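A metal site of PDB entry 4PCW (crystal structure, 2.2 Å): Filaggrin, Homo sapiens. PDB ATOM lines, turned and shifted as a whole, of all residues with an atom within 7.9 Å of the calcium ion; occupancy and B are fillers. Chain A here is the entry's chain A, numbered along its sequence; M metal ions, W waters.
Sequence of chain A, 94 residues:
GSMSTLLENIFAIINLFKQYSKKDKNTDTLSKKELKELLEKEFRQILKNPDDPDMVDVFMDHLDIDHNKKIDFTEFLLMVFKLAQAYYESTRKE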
ATOM      1  N   THR A  29      26.084 -15.515  14.210  1.00  0.00           N
ATOM      2  CA  THR A  29      25.926 -14.829  15.491  1.00  0.00           C
ATOM      3  C   THR A  29      24.518 -14.270  15.639  1.00  0.00           C
ATOM      4  O   THR A  29      23.823 -14.050  14.645  1.00  0.00           O
ATOM      5  CB  THR A  29      26.922 -13.658  15.644  1.00  0.00           C
ATOM      6  OG1 THR A  29      26.700 -12.683  14.621  1.00  0.00           O
ATOM      7  CG2 THR A  29      28.360 -14.142  15.591  1.00  0.00           C
ATOM      8  N   LEU A  30      24.111 -14.035  16.883  1.00  0.00           N
ATOM      9  CA  LEU A  30      22.839 -13.386  17.171  1.00  0.00           C
ATOM     10  C   LEU A  30      23.051 -11.899  17.420  1.00  0.00           C
ATOM     11  O   LEU A  30      23.886 -11.508  18.242  1.00  0.00           O
ATOM     12  CB  LEU A  30      22.154 -14.023  18.394  1.00  0.00           C
ATOM     13  CG  LEU A  30      21.792 -15.500  18.316  1.00  0.00           C
ATOM     14  CD1 LEU A  30      21.641 -16.086  19.715  1.00  0.00           C
ATOM     15  CD2 LEU A  30      20.513 -15.683  17.518  1.00  0.00           C
ATOM     16  N   MET A  60      22.182  -9.186  26.878  1.00  0.00           N
ATOM     17  CA  MET A  60      23.150  -9.092  25.793  1.00  0.00           C
ATOM     18  C   MET A  60      24.572  -8.959  26.357  1.00  0.00           C
ATOM     19  O   MET A  60      25.514  -9.562  25.848  1.00  0.00           O
ATOM     20  CB  MET A  60      22.812  -7.920  24.881  1.00  0.00           C
ATOM     21  CG  MET A  60      23.672  -7.820  23.634  1.00  0.00           C
ATOM     22  SD  MET A  60      23.280  -9.090  22.425  1.00  0.00           S
ATOM     23  CE  MET A  60      24.344  -8.604  21.065  1.00  0.00           C
ATOM     24  N   LEU A  63      25.980 -12.309  28.038  1.00  0.00           N
ATOM     25  CA  LEU A  63      26.444 -13.329  27.095  1.00  0.00           C
ATOM     26  C   LEU A  63      27.622 -12.860  26.239  1.00  0.00           C
ATOM     27  O   LEU A  63      28.477 -13.663  25.867  1.00  0.00           O
ATOM     28  CB  LEU A  63      25.288 -13.743  26.173  1.00  0.00           C
ATOM     29  CG  LEU A  63      24.308 -14.792  26.703  1.00  0.00           C
ATOM     30  CD1 LEU A  63      23.709 -14.372  28.044  1.00  0.00           C
ATOM     31  CD2 LEU A  63      23.211 -15.016  25.673  1.00  0.00           C
ATOM     32  N   ASP A  64      27.642 -11.572  25.928  1.00  0.00           N
ATOM     33  CA  ASP A  64      28.653 -11.020  25.031  1.00  0.00           C
ATOM     34  C   ASP A  64      29.969 -10.787  25.762  1.00  0.00           C
ATOM     35  O   ASP A  64      30.316  -9.655  26.097  1.00  0.00           O
ATOM     36  CB  ASP A  64      28.146  -9.708  24.423  1.00  0.00           C
ATOM     37  CG  ASP A  64      29.052  -9.181  23.335  1.00  0.00           C
ATOM     38  OD1 ASP A  64      29.825  -9.978  22.753  1.00  0.00           O
ATOM     39  OD2 ASP A  64      28.984  -7.969  23.048  1.00  0.00           O
ATOM     40  N   ILE A  65      30.726 -11.863  25.978  1.00  0.00           N
ATOM     41  CA  ILE A  65      31.909 -11.810  26.843  1.00  0.00           C
ATOM     42  C   ILE A  65      33.189 -11.394  26.109  1.00  0.00           C
ATOM     43  O   ILE A  65      34.227 -11.229  26.743  1.00  0.00           O
ATOM     44  CB  ILE A  65      32.152 -13.167  27.527  1.00  0.00           C
ATOM     45  CG1 ILE A  65      32.401 -14.268  26.490  1.00  0.00           C
ATOM     46  CG2 ILE A  65      30.955 -13.516  28.408  1.00  0.00           C
ATOM     47  CD1 ILE A  65      32.801 -15.595  27.104  1.00  0.00           C
ATOM     48  N   ASP A  66      33.120 -11.240  24.788  1.00  0.00           N
ATOM     49  CA  ASP A  66      34.225 -10.646  24.031  1.00  0.00           C
ATOM     50  C   ASP A  66      33.884  -9.212  23.609  1.00  0.00           C
ATOM     51  O   ASP A  66      34.727  -8.506  23.049  1.00  0.00           O
ATOM     52  CB  ASP A  66      34.566 -11.500  22.808  1.00  0.00           C
ATOM     53  CG  ASP A  66      33.393 -11.693  21.864  1.00  0.00           C
ATOM     54  OD1 ASP A  66      32.388 -10.974  21.989  1.00  0.00           O
ATOM     55  OD2 ASP A  66      33.487 -12.580  20.988  1.00  0.00           O
ATOM     56  N   HIS A  67      32.653  -8.807  23.870  1.00  0.00           N
ATOM     57  CA  HIS A  67      32.212  -7.424  23.656  1.00  0.00           C
ATOM     58  C   HIS A  67      32.321  -6.975  22.198  1.00  0.00           C
ATOM     59  O   HIS A  67      32.994  -5.992  21.898  1.00  0.00           O
ATOM     60  CB  HIS A  67      33.021  -6.483  24.546  1.00  0.00           C
ATOM     61  CG  HIS A  67      33.028  -6.864  25.992  1.00  0.00           C
ATOM     62  ND1 HIS A  67      34.109  -7.458  26.600  1.00  0.00           N
ATOM     63  CD2 HIS A  67      32.074  -6.736  26.947  1.00  0.00           C
ATOM     64  CE1 HIS A  67      33.830  -7.676  27.874  1.00  0.00           C
ATOM     65  NE2 HIS A  67      32.604  -7.253  28.109  1.00  0.00           N
ATOM     66  N   ASN A  68      31.645  -7.698  21.297  1.00  0.00           N
ATOM     67  CA  ASN A  68      31.577  -7.304  19.885  1.00  0.00           C
ATOM     68  C   ASN A  68      30.131  -7.116  19.411  1.00  0.00           C
ATOM     69  O   ASN A  68      29.859  -7.121  18.217  1.00  0.00           O
ATOM     70  CB  ASN A  68      32.283  -8.350  19.006  1.00  0.00           C
ATOM     71  CG  ASN A  68      31.634  -9.715  19.084  1.00  0.00           C
ATOM     72  OD1 ASN A  68      30.647  -9.918  19.784  1.00  0.00           O
ATOM     73  ND2 ASN A  68      32.200 -10.669  18.349  1.00  0.00           N
ATOM     74  N   LYS A  69      29.222  -6.929  20.371  1.00  0.00           N
ATOM     75  CA  LYS A  69      27.801  -6.671  20.089  1.00  0.00           C
ATOM     76  C   LYS A  69      27.107  -7.801  19.321  1.00  0.00           C
ATOM     77  O   LYS A  69      26.057  -7.597  18.707  1.00  0.00           O
ATOM     78  CB  LYS A  69      27.645  -5.354  19.308  1.00  0.00           C
ATOM     79  CG  LYS A  69      27.922  -4.114  20.129  1.00  0.00           C
ATOM     80  CD  LYS A  69      27.542  -2.832  19.389  1.00  0.00           C
ATOM     81  CE  LYS A  69      26.077  -2.436  19.610  1.00  0.00           C
ATOM     82  NZ  LYS A  69      25.098  -3.277  18.850  1.00  0.00           N
ATOM     83  N   LYS A  70      27.685  -8.999  19.356  1.00  0.00           N
ATOM     84  CA  LYS A  70      27.087 -10.166  18.728  1.00  0.00           C
ATOM     85  C   LYS A  70      27.276 -11.400  19.609  1.00  0.00           C
ATOM     86  O   LYS A  70      28.266 -11.494  20.334  1.00  0.00           O
ATOM     87  CB  LYS A  70      27.689 -10.416  17.350  1.00  0.00           C
ATOM     88  CG  LYS A  70      27.118  -9.520  16.246  1.00  0.00           C
ATOM     89  CD  LYS A  70      28.177  -8.610  15.651  1.00  0.00           C
ATOM     90  CE  LYS A  70      29.235  -9.379  14.883  1.00  0.00           C
ATOM     91  NZ  LYS A  70      30.580  -8.737  14.966  1.00  0.00           N
ATOM     92  N   ILE A  71      26.338 -12.339  19.534  1.00  0.00           N
ATOM     93  CA  ILE A  71      26.405 -13.550  20.343  1.00  0.00           C
ATOM     94  C   ILE A  71      26.654 -14.759  19.467  1.00  0.00           C
ATOM     95  O   ILE A  71      25.744 -15.259  18.810  1.00  0.00           O
ATOM     96  CB  ILE A  71      25.104 -13.767  21.155  1.00  0.00           C
ATOM     97  CG1 ILE A  71      24.734 -12.505  21.937  1.00  0.00           C
ATOM     98  CG2 ILE A  71      25.240 -14.950  22.082  1.00  0.00           C
ATOM     99  CD1 ILE A  71      25.794 -12.028  22.911  1.00  0.00           C
ATOM    100  N   ASP A  72      27.903 -15.227  19.437  1.00  0.00           N
ATOM    101  CA  ASP A  72      28.234 -16.412  18.660  1.00  0.00           C
ATOM    102  C   ASP A  72      27.721 -17.654  19.378  1.00  0.00           C
ATOM    103  O   ASP A  72      27.182 -17.564  20.481  1.00  0.00           O
ATOM    104  CB  ASP A  72      29.737 -16.509  18.389  1.00  0.00           C
ATOM    105  CG  ASP A  72      30.582 -16.495  19.656  1.00  0.00           C
ATOM    106  OD1 ASP A  72      30.224 -17.175  20.643  1.00  0.00           O
ATOM    107  OD2 ASP A  72      31.614 -15.791  19.664  1.00  0.00           O
ATOM    108  N   PHE A  73      27.884 -18.814  18.743  1.00  0.00           N
ATOM    109  CA  PHE A  73      27.313 -20.049  19.253  1.00  0.00           C
ATOM    110  C   PHE A  73      27.939 -20.425  20.596  1.00  0.00           C
ATOM    111  O   PHE A  73      27.245 -20.884  21.500  1.00  0.00           O
ATOM    112  CB  PHE A  73      27.492 -21.178  18.237  1.00  0.00           C
ATOM    113  CG  PHE A  73      26.739 -22.435  18.577  1.00  0.00           C
ATOM    114  CD1 PHE A  73      25.362 -22.397  18.739  1.00  0.00           C
ATOM    115  CD2 PHE A  73      27.406 -23.638  18.713  1.00  0.00           C
ATOM    116  CE1 PHE A  73      24.664 -23.559  19.046  1.00  0.00           C
ATOM    117  CE2 PHE A  73      26.712 -24.796  19.012  1.00  0.00           C
ATOM    118  CZ  PHE A  73      25.338 -24.750  19.180  1.00  0.00           C
ATOM    119  N   GLU A  75      29.217 -18.477  22.972  1.00  0.00           N
ATOM    120  CA  GLU A  75      28.636 -17.628  24.013  1.00  0.00           C
ATOM    121  C   GLU A  75      27.206 -18.049  24.325  1.00  0.00           C
ATOM    122  O   GLU A  75      26.759 -17.986  25.469  1.00  0.00           O
ATOM    123  CB  GLU A  75      28.672 -16.168  23.585  1.00  0.00           C
ATOM    124  CG  GLU A  75      30.067 -15.581  23.542  1.00  0.00           C
ATOM    125  CD  GLU A  75      30.091 -14.194  22.956  1.00  0.00           C
ATOM    126  OE1 GLU A  75      29.313 -13.927  22.013  1.00  0.00           O
ATOM    127  OE2 GLU A  75      30.880 -13.357  23.436  1.00  0.00           O
HETATM  128 CA    CA M   1      30.340 -11.788  21.212  1.00  0.00          CA
HETATM  129  O   HOH W   1      31.706 -13.426  19.956  1.00  0.00           O
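Five residues have an atom within 4 Å of the calcium ion: Asp 64, Asp 66, Asn 68, Lys 70 and Glu 75.
Along chain A the residues within 4 Å of the calcium ion span positions 64 to 75.
The nearest printed residue that does not touch the calcium ion is Ile 71 (4.4 Å).
The calcium ion is bound by O of Lys 70 (2.3 Å), OD1 of Asp 66 (2.3 Å), OD1 of Asn 68 (2.4 Å), OD1 of Asp 64 (2.4 Å), water W1 (2.5 Å), OE1 of Glu 75 (2.5 Å) and OE2 of Glu 75 (2.8 Å).
The side-chain carboxylate (OE2) of Glu 75 sits close to the backbone NH (N) of Ile 65.
The side-chain carboxylate (OD1) of Asp 64 sits close to the backbone NH (N) of His 67 (3.3 Å).
The side-chain carboxylate (OD1) of Asp 72 is in hydrogen-bond range of the backbone NH (N) of Glu 75.
The backbone NH of Lys 69 sits at hydrogen-bond distance from the side-chain carboxylate of Asp 64, at 2.9 Å.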
